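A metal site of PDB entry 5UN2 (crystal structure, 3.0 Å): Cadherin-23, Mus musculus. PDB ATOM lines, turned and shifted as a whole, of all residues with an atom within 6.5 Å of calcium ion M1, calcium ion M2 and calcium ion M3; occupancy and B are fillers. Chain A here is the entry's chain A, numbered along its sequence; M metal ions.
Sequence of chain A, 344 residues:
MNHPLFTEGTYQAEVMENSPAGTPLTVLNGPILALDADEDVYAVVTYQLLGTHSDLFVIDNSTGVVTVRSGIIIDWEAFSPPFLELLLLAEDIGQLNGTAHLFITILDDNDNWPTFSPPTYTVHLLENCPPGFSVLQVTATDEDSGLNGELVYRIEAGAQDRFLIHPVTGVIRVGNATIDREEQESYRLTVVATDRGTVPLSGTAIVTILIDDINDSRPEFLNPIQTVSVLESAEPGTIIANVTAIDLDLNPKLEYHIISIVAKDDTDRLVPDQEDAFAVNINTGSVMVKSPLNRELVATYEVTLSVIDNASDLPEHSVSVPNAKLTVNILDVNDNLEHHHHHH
Four residues have an atom within 4 Å of calcium ion M2: Glu 127, Asp 180, Glu 182 and Asp 216.
OG of Ser 312 is in hydrogen-bond range of O of Asp 309, at 3.3 Å. N of Asp 309 lies within hydrogen-bond range of O of Ser 318 (2.9 Å). ND2 of Asn 215 sits close to O of Ala 311 (3.1 Å). The backbone NH of Ser 312 sits close to the side-chain amide nitrogen of Asn 215. OD2 of Asp 216 sits close to ND2 of Asn 128 (3.1 Å). O of Asn 215 lies within hydrogen-bond range of N of Asp 313 (2.6 Å). OD2 of Asp 213 sits at hydrogen-bond distance from N of Leu 250, at 3.4 Å. The guanidinium group (NE) of Arg 181 sits close to the side-chain carboxylate (OD1) of Asp 213 (3.2 Å).
O of Ser 217 binds calcium ion M3, at 2.4 Å. Calcium ion M3 is bound by OD1 of Asn 215. Calcium ion M3 is bound by OD2 of Asp 247 (2.4 Å). The side-chain carboxylate (OD2) of Asp 249 binds calcium ion M3 (2.5 Å). The side-chain carboxylate (OD1) of Asp 247 binds calcium ion M3 (2.7 Å). The side-chain carboxylate (OD2) of Asp 309 binds calcium ion M3 (2.7 Å). Calcium ion M3 has six donor atoms within binding distance.
Merely in contact with calcium ion M3: Ser 312 and His 317. Seven residues have an atom within 4 Å of calcium ion M3: Asn 215, Ser 217, Asp 247, Asp 249, Asp 309, Ser 312 and His 317. The nearest printed residue that does not touch calcium ion M3 is Arg 218 (4.3 Å).
The backbone carbonyl oxygen (O) of Ile 214 binds calcium ion M1 (2.2 Å). Calcium ion M1 is bound by the side-chain carboxylate (OD1) of Asp 249 (2.4 Å). OE1 of Glu 127 binds calcium ion M1 (2.4 Å). OE2 of Glu 182 binds calcium ion M1, 2.4 Å away. Calcium ion M1 is bound by OE1 of Glu 182. Calcium ion M1 is bound by OD1 of Asp 216, at 2.6 Å. OD1 of Asp 213 is bound to calcium ion M1. Calcium ion M1 has seven donor atoms within binding distance.
The nearest printed residue that does not touch calcium ion M1 is Asn 215 (4.3 Å).
Calcium ion M2 is bound by the side-chain carboxylate (OD1) of Asp 180 (2.3 Å), the side-chain carboxylate (OE2) of Glu 127 (2.4 Å), the side-chain carboxylate (OE1) of Glu 182 (2.5 Å), the side-chain carboxylate (OD2) of Asp 216 (2.7 Å) and the side-chain carboxylate (OD1) of Asp 216 (2.7 Å).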
ATOM      1  N   GLU A 127      -6.274 -26.563  -5.499  1.00  0.00           N
ATOM      2  CA  GLU A 127      -4.831 -26.380  -5.350  1.00  0.00           C
ATOM      3  C   GLU A 127      -4.507 -25.827  -3.965  1.00  0.00           C
ATOM      4  O   GLU A 127      -5.412 -25.365  -3.247  1.00  0.00           O
ATOM      5  CB  GLU A 127      -4.267 -25.489  -6.465  1.00  0.00           C
ATOM      6  CG  GLU A 127      -4.679 -24.019  -6.450  1.00  0.00           C
ATOM      7  CD  GLU A 127      -3.959 -23.209  -7.520  1.00  0.00           C
ATOM      8  OE1 GLU A 127      -4.645 -22.555  -8.346  1.00  0.00           O
ATOM      9  OE2 GLU A 127      -2.697 -23.215  -7.556  1.00  0.00           O
ATOM     10  N   ASN A 128      -3.211 -25.890  -3.589  1.00  0.00           N
ATOM     11  CA  ASN A 128      -2.712 -25.528  -2.226  1.00  0.00           C
ATOM     12  C   ASN A 128      -3.370 -26.337  -1.110  1.00  0.00           C
ATOM     13  O   ASN A 128      -3.474 -25.842   0.016  1.00  0.00           O
ATOM     14  CB  ASN A 128      -2.892 -24.029  -1.894  1.00  0.00           C
ATOM     15  CG  ASN A 128      -2.562 -23.111  -3.040  1.00  0.00           C
ATOM     16  OD1 ASN A 128      -1.611 -23.329  -3.786  1.00  0.00           O
ATOM     17  ND2 ASN A 128      -3.369 -22.059  -3.187  1.00  0.00           N
ATOM     18  N   ILE A 179       0.502 -29.016  -4.556  1.00  0.00           N
ATOM     19  CA  ILE A 179      -0.360 -29.209  -5.747  1.00  0.00           C
ATOM     20  C   ILE A 179      -0.710 -27.846  -6.366  1.00  0.00           C
ATOM     21  O   ILE A 179      -1.625 -27.168  -5.895  1.00  0.00           O
ATOM     22  CB  ILE A 179      -1.668 -29.986  -5.441  1.00  0.00           C
ATOM     23  CG1 ILE A 179      -1.357 -31.313  -4.720  1.00  0.00           C
ATOM     24  CG2 ILE A 179      -2.484 -30.207  -6.726  1.00  0.00           C
ATOM     25  CD1 ILE A 179      -0.248 -32.135  -5.362  1.00  0.00           C
ATOM     26  N   ASP A 180       0.024 -27.492  -7.426  1.00  0.00           N
ATOM     27  CA  ASP A 180      -0.072 -26.179  -8.086  1.00  0.00           C
ATOM     28  C   ASP A 180      -0.746 -26.319  -9.441  1.00  0.00           C
ATOM     29  O   ASP A 180      -0.201 -26.980 -10.329  1.00  0.00           O
ATOM     30  CB  ASP A 180       1.337 -25.604  -8.266  1.00  0.00           C
ATOM     31  CG  ASP A 180       1.350 -24.175  -8.751  1.00  0.00           C
ATOM     32  OD1 ASP A 180       0.260 -23.568  -8.903  1.00  0.00           O
ATOM     33  OD2 ASP A 180       2.464 -23.644  -8.933  1.00  0.00           O
ATOM     34  N   ARG A 181      -1.924 -25.709  -9.617  1.00  0.00           N
ATOM     35  CA  ARG A 181      -2.665 -25.830 -10.874  1.00  0.00           C
ATOM     36  C   ARG A 181      -1.843 -25.265 -12.026  1.00  0.00           C
ATOM     37  O   ARG A 181      -1.894 -25.789 -13.135  1.00  0.00           O
ATOM     38  CB  ARG A 181      -4.034 -25.119 -10.824  1.00  0.00           C
ATOM     39  CG  ARG A 181      -5.030 -25.627 -11.890  1.00  0.00           C
ATOM     40  CD  ARG A 181      -6.113 -24.609 -12.245  1.00  0.00           C
ATOM     41  NE  ARG A 181      -5.542 -23.359 -12.757  1.00  0.00           N
ATOM     42  CZ  ARG A 181      -5.203 -23.097 -14.022  1.00  0.00           C
ATOM     43  NH1 ARG A 181      -4.674 -21.914 -14.321  1.00  0.00           N
ATOM     44  NH2 ARG A 181      -5.383 -23.985 -15.000  1.00  0.00           N
ATOM     45  N   GLU A 182      -1.073 -24.226 -11.733  1.00  0.00           N
ATOM     46  CA  GLU A 182      -0.225 -23.560 -12.743  1.00  0.00           C
ATOM     47  C   GLU A 182       0.987 -24.427 -13.182  1.00  0.00           C
ATOM     48  O   GLU A 182       1.471 -24.273 -14.301  1.00  0.00           O
ATOM     49  CB  GLU A 182       0.213 -22.167 -12.252  1.00  0.00           C
ATOM     50  CG  GLU A 182      -0.894 -21.105 -12.272  1.00  0.00           C
ATOM     51  CD  GLU A 182      -2.039 -21.326 -11.261  1.00  0.00           C
ATOM     52  OE1 GLU A 182      -1.810 -21.572 -10.043  1.00  0.00           O
ATOM     53  OE2 GLU A 182      -3.211 -21.210 -11.668  1.00  0.00           O
ATOM     54  N   GLU A 183       1.445 -25.326 -12.309  1.00  0.00           N
ATOM     55  CA  GLU A 183       2.564 -26.256 -12.586  1.00  0.00           C
ATOM     56  C   GLU A 183       2.108 -27.568 -13.220  1.00  0.00           C
ATOM     57  O   GLU A 183       2.857 -28.190 -13.981  1.00  0.00           O
ATOM     58  CB  GLU A 183       3.329 -26.547 -11.289  1.00  0.00           C
ATOM     59  CG  GLU A 183       4.747 -27.101 -11.459  1.00  0.00           C
ATOM     60  CD  GLU A 183       4.851 -28.619 -11.372  1.00  0.00           C
ATOM     61  OE1 GLU A 183       5.927 -29.152 -11.773  1.00  0.00           O
ATOM     62  OE2 GLU A 183       3.885 -29.271 -10.921  1.00  0.00           O
ATOM     63  N   ASP A 212      -8.569 -27.772  -9.608  1.00  0.00           N
ATOM     64  CA  ASP A 212      -9.364 -26.547  -9.679  1.00  0.00           C
ATOM     65  C   ASP A 212      -8.470 -25.362  -9.333  1.00  0.00           C
ATOM     66  O   ASP A 212      -7.373 -25.539  -8.797  1.00  0.00           O
ATOM     67  CB  ASP A 212     -10.577 -26.624  -8.719  1.00  0.00           C
ATOM     68  CG  ASP A 212     -11.639 -27.640  -9.186  1.00  0.00           C
ATOM     69  OD1 ASP A 212     -11.508 -28.209 -10.296  1.00  0.00           O
ATOM     70  OD2 ASP A 212     -12.626 -27.857  -8.449  1.00  0.00           O
ATOM     71  N   ASP A 213      -8.957 -24.165  -9.637  1.00  0.00           N
ATOM     72  CA  ASP A 213      -8.187 -22.924  -9.502  1.00  0.00           C
ATOM     73  C   ASP A 213      -8.507 -22.121  -8.248  1.00  0.00           C
ATOM     74  O   ASP A 213      -9.663 -21.914  -7.900  1.00  0.00           O
ATOM     75  CB  ASP A 213      -8.436 -22.031 -10.730  1.00  0.00           C
ATOM     76  CG  ASP A 213      -7.549 -20.780 -10.738  1.00  0.00           C
ATOM     77  OD1 ASP A 213      -6.296 -20.919 -10.836  1.00  0.00           O
ATOM     78  OD2 ASP A 213      -8.114 -19.653 -10.680  1.00  0.00           O
ATOM     79  N   ILE A 214      -7.437 -21.672  -7.592  1.00  0.00           N
ATOM     80  CA  ILE A 214      -7.453 -20.510  -6.720  1.00  0.00           C
ATOM     81  C   ILE A 214      -6.619 -19.454  -7.448  1.00  0.00           C
ATOM     82  O   ILE A 214      -5.545 -19.781  -7.993  1.00  0.00           O
ATOM     83  CB  ILE A 214      -6.802 -20.831  -5.364  1.00  0.00           C
ATOM     84  CG1 ILE A 214      -7.486 -22.033  -4.706  1.00  0.00           C
ATOM     85  CG2 ILE A 214      -6.837 -19.622  -4.441  1.00  0.00           C
ATOM     86  CD1 ILE A 214      -7.026 -22.278  -3.284  1.00  0.00           C
ATOM     87  N   ASN A 215      -7.108 -18.212  -7.508  1.00  0.00           N
ATOM     88  CA  ASN A 215      -6.406 -17.131  -8.216  1.00  0.00           C
ATOM     89  C   ASN A 215      -5.282 -16.670  -7.316  1.00  0.00           C
ATOM     90  O   ASN A 215      -5.467 -15.750  -6.517  1.00  0.00           O
ATOM     91  CB  ASN A 215      -7.386 -16.002  -8.592  1.00  0.00           C
ATOM     92  CG  ASN A 215      -6.792 -14.977  -9.556  1.00  0.00           C
ATOM     93  OD1 ASN A 215      -5.579 -14.805  -9.653  1.00  0.00           O
ATOM     94  ND2 ASN A 215      -7.674 -14.254 -10.248  1.00  0.00           N
ATOM     95  N   ASP A 216      -4.129 -17.334  -7.442  1.00  0.00           N
ATOM     96  CA  ASP A 216      -3.035 -17.277  -6.458  1.00  0.00           C
ATOM     97  C   ASP A 216      -1.641 -17.018  -7.057  1.00  0.00           C
ATOM     98  O   ASP A 216      -0.626 -17.217  -6.381  1.00  0.00           O
ATOM     99  CB  ASP A 216      -3.020 -18.577  -5.635  1.00  0.00           C
ATOM    100  CG  ASP A 216      -2.565 -19.801  -6.443  1.00  0.00           C
ATOM    101  OD1 ASP A 216      -2.432 -19.720  -7.699  1.00  0.00           O
ATOM    102  OD2 ASP A 216      -2.316 -20.871  -5.819  1.00  0.00           O
ATOM    103  N   SER A 217      -1.612 -16.555  -8.301  1.00  0.00           N
ATOM    104  CA  SER A 217      -0.362 -16.405  -9.064  1.00  0.00           C
ATOM    105  C   SER A 217      -0.275 -15.001  -9.674  1.00  0.00           C
ATOM    106  O   SER A 217      -1.151 -14.622 -10.466  1.00  0.00           O
ATOM    107  CB  SER A 217      -0.316 -17.478 -10.151  1.00  0.00           C
ATOM    108  OG  SER A 217       0.662 -17.191 -11.108  1.00  0.00           O
ATOM    109  N   ARG A 218       0.760 -14.256  -9.288  1.00  0.00           N
ATOM    110  CA  ARG A 218       0.866 -12.831  -9.642  1.00  0.00           C
ATOM    111  C   ARG A 218       1.060 -12.615 -11.138  1.00  0.00           C
ATOM    112  O   ARG A 218       1.716 -13.431 -11.797  1.00  0.00           O
ATOM    113  CB  ARG A 218       2.000 -12.137  -8.867  1.00  0.00           C
ATOM    114  CG  ARG A 218       3.414 -12.496  -9.344  1.00  0.00           C
ATOM    115  CD  ARG A 218       4.497 -11.715  -8.617  1.00  0.00           C
ATOM    116  NE  ARG A 218       4.616 -12.140  -7.230  1.00  0.00           N
ATOM    117  CZ  ARG A 218       4.043 -11.553  -6.190  1.00  0.00           C
ATOM    118  NH1 ARG A 218       4.250 -12.088  -4.979  1.00  0.00           N
ATOM    119  NH2 ARG A 218       3.287 -10.454  -6.311  1.00  0.00           N
ATOM    120  N   PRO A 219       0.505 -11.516 -11.670  1.00  0.00           N
ATOM    121  CA  PRO A 219       0.779 -11.213 -13.074  1.00  0.00           C
ATOM    122  C   PRO A 219       2.277 -10.969 -13.320  1.00  0.00           C
ATOM    123  O   PRO A 219       3.008 -10.507 -12.420  1.00  0.00           O
ATOM    124  CB  PRO A 219      -0.038  -9.955 -13.330  1.00  0.00           C
ATOM    125  CG  PRO A 219      -0.130  -9.305 -11.995  1.00  0.00           C
ATOM    126  CD  PRO A 219      -0.282 -10.446 -11.036  1.00  0.00           C
ATOM    127  N   ASP A 247      -1.118 -13.418 -16.394  1.00  0.00           N
ATOM    128  CA  ASP A 247      -1.487 -14.078 -15.137  1.00  0.00           C
ATOM    129  C   ASP A 247      -1.870 -15.515 -15.528  1.00  0.00           C
ATOM    130  O   ASP A 247      -2.688 -15.719 -16.420  1.00  0.00           O
ATOM    131  CB  ASP A 247      -2.690 -13.328 -14.497  1.00  0.00           C
ATOM    132  CG  ASP A 247      -2.926 -13.651 -12.981  1.00  0.00           C
ATOM    133  OD1 ASP A 247      -3.532 -14.678 -12.618  1.00  0.00           O
ATOM    134  OD2 ASP A 247      -2.556 -12.808 -12.121  1.00  0.00           O
ATOM    135  N   LEU A 248      -1.272 -16.512 -14.888  1.00  0.00           N
ATOM    136  CA  LEU A 248      -1.499 -17.901 -15.309  1.00  0.00           C
ATOM    137  C   LEU A 248      -2.723 -18.529 -14.655  1.00  0.00           C
ATOM    138  O   LEU A 248      -2.990 -19.702 -14.895  1.00  0.00           O
ATOM    139  CB  LEU A 248      -0.256 -18.771 -15.049  1.00  0.00           C
ATOM    140  CG  LEU A 248       1.060 -18.252 -15.639  1.00  0.00           C
ATOM    141  CD1 LEU A 248       2.259 -19.040 -15.155  1.00  0.00           C
ATOM    142  CD2 LEU A 248       1.016 -18.241 -17.159  1.00  0.00           C
ATOM    143  N   ASP A 249      -3.462 -17.755 -13.844  1.00  0.00           N
ATOM    144  CA  ASP A 249      -4.697 -18.249 -13.178  1.00  0.00           C
ATOM    145  C   ASP A 249      -5.874 -18.251 -14.152  1.00  0.00           C
ATOM    146  O   ASP A 249      -5.759 -17.735 -15.264  1.00  0.00           O
ATOM    147  CB  ASP A 249      -5.046 -17.398 -11.958  1.00  0.00           C
ATOM    148  CG  ASP A 249      -3.967 -17.388 -10.923  1.00  0.00           C
ATOM    149  OD1 ASP A 249      -3.599 -18.486 -10.478  1.00  0.00           O
ATOM    150  OD2 ASP A 249      -3.505 -16.292 -10.545  1.00  0.00           O
ATOM    151  N   LEU A 250      -7.006 -18.780 -13.720  1.00  0.00           N
ATOM    152  CA  LEU A 250      -8.076 -19.109 -14.659  1.00  0.00           C
ATOM    153  C   LEU A 250      -8.902 -17.932 -15.184  1.00  0.00           C
ATOM    154  O   LEU A 250      -9.317 -17.948 -16.348  1.00  0.00           O
ATOM    155  CB  LEU A 250      -8.982 -20.195 -14.093  1.00  0.00           C
ATOM    156  CG  LEU A 250      -9.362 -21.308 -15.067  1.00  0.00           C
ATOM    157  CD1 LEU A 250      -8.123 -22.000 -15.628  1.00  0.00           C
ATOM    158  CD2 LEU A 250     -10.281 -22.303 -14.361  1.00  0.00           C
ATOM    159  N   PRO A 252      -8.373 -14.008 -14.844  1.00  0.00           N
ATOM    160  CA  PRO A 252      -7.764 -12.774 -14.331  1.00  0.00           C
ATOM    161  C   PRO A 252      -8.497 -11.546 -14.797  1.00  0.00           C
ATOM    162  O   PRO A 252      -9.137 -11.583 -15.830  1.00  0.00           O
ATOM    163  CB  PRO A 252      -6.355 -12.798 -14.930  1.00  0.00           C
ATOM    164  CG  PRO A 252      -6.235 -14.065 -15.698  1.00  0.00           C
ATOM    165  CD  PRO A 252      -7.619 -14.534 -15.984  1.00  0.00           C
ATOM    166  N   LEU A 254      -6.832  -8.162 -15.320  1.00  0.00           N
ATOM    167  CA  LEU A 254      -5.644  -7.322 -15.245  1.00  0.00           C
ATOM    168  C   LEU A 254      -5.942  -5.849 -15.403  1.00  0.00           C
ATOM    169  O   LEU A 254      -6.764  -5.457 -16.214  1.00  0.00           O
ATOM    170  CB  LEU A 254      -4.590  -7.744 -16.261  1.00  0.00           C
ATOM    171  CG  LEU A 254      -3.599  -8.820 -15.790  1.00  0.00           C
ATOM    172  CD1 LEU A 254      -4.333  -9.979 -15.125  1.00  0.00           C
ATOM    173  CD2 LEU A 254      -2.750  -9.316 -16.957  1.00  0.00           C
ATOM    174  N   ASP A 309      -3.855  -8.196 -10.703  1.00  0.00           N
ATOM    175  CA  ASP A 309      -5.002  -9.059 -10.942  1.00  0.00           C
ATOM    176  C   ASP A 309      -6.089  -8.781  -9.879  1.00  0.00           C
ATOM    177  O   ASP A 309      -5.967  -9.245  -8.745  1.00  0.00           O
ATOM    178  CB  ASP A 309      -4.587 -10.535 -10.923  1.00  0.00           C
ATOM    179  CG  ASP A 309      -5.682 -11.480 -11.422  1.00  0.00           C
ATOM    180  OD1 ASP A 309      -6.791 -10.986 -11.733  1.00  0.00           O
ATOM    181  OD2 ASP A 309      -5.418 -12.704 -11.517  1.00  0.00           O
ATOM    182  N   ALA A 311      -8.969  -9.997  -9.655  1.00  0.00           N
ATOM    183  CA  ALA A 311      -9.626 -11.233  -9.266  1.00  0.00           C
ATOM    184  C   ALA A 311      -8.805 -12.081  -8.293  1.00  0.00           C
ATOM    185  O   ALA A 311      -9.313 -13.097  -7.824  1.00  0.00           O
ATOM    186  CB  ALA A 311      -9.972 -12.049 -10.500  1.00  0.00           C
ATOM    187  N   SER A 312      -7.561 -11.704  -7.978  1.00  0.00           N
ATOM    188  CA  SER A 312      -6.696 -12.598  -7.207  1.00  0.00           C
ATOM    189  C   SER A 312      -7.231 -12.855  -5.778  1.00  0.00           C
ATOM    190  O   SER A 312      -7.635 -11.934  -5.061  1.00  0.00           O
ATOM    191  CB  SER A 312      -5.224 -12.161  -7.189  1.00  0.00           C
ATOM    192  OG  SER A 312      -4.976 -11.177  -6.199  1.00  0.00           O
ATOM    193  N   ASP A 313      -7.253 -14.141  -5.419  1.00  0.00           N
ATOM    194  CA  ASP A 313      -7.778 -14.588  -4.146  1.00  0.00           C
ATOM    195  C   ASP A 313      -6.722 -14.360  -3.047  1.00  0.00           C
ATOM    196  O   ASP A 313      -7.085 -14.203  -1.913  1.00  0.00           O
ATOM    197  CB  ASP A 313      -8.213 -16.066  -4.213  1.00  0.00           C
ATOM    198  CG  ASP A 313      -9.444 -16.307  -5.132  1.00  0.00           C
ATOM    199  OD1 ASP A 313     -10.463 -15.595  -5.026  1.00  0.00           O
ATOM    200  OD2 ASP A 313      -9.413 -17.247  -5.968  1.00  0.00           O
ATOM    201  N   HIS A 317      -0.090 -12.011  -3.940  1.00  0.00           N
ATOM    202  CA  HIS A 317       0.176 -12.334  -5.361  1.00  0.00           C
ATOM    203  C   HIS A 317      -0.756 -11.572  -6.300  1.00  0.00           C
ATOM    204  O   HIS A 317      -1.347 -12.133  -7.253  1.00  0.00           O
ATOM    205  CB  HIS A 317       0.035 -13.831  -5.562  1.00  0.00           C
ATOM    206  CG  HIS A 317       0.921 -14.622  -4.674  1.00  0.00           C
ATOM    207  ND1 HIS A 317       2.215 -14.955  -5.010  1.00  0.00           N
ATOM    208  CD2 HIS A 317       0.707 -15.153  -3.443  1.00  0.00           C
ATOM    209  CE1 HIS A 317       2.757 -15.655  -4.032  1.00  0.00           C
ATOM    210  NE2 HIS A 317       1.860 -15.781  -3.067  1.00  0.00           N
ATOM    211  N   SER A 318      -0.901 -10.283  -6.001  1.00  0.00           N
ATOM    212  CA  SER A 318      -1.833  -9.418  -6.694  1.00  0.00           C
ATOM    213  C   SER A 318      -1.140  -8.668  -7.794  1.00  0.00           C
ATOM    214  O   SER A 318      -1.674  -8.529  -8.890  1.00  0.00           O
ATOM    215  CB  SER A 318      -2.403  -8.390  -5.730  1.00  0.00           C
ATOM    216  OG  SER A 318      -3.302  -8.996  -4.844  1.00  0.00           O
HETATM  217 CA    CA M   1      -4.072 -20.569  -9.489  1.00  0.00          CA
HETATM  218 CA    CA M   2      -0.786 -21.846  -7.797  1.00  0.00          CA
HETATM  219 CA    CA M   3      -3.398 -13.861 -10.100  1.00  0.00          CA
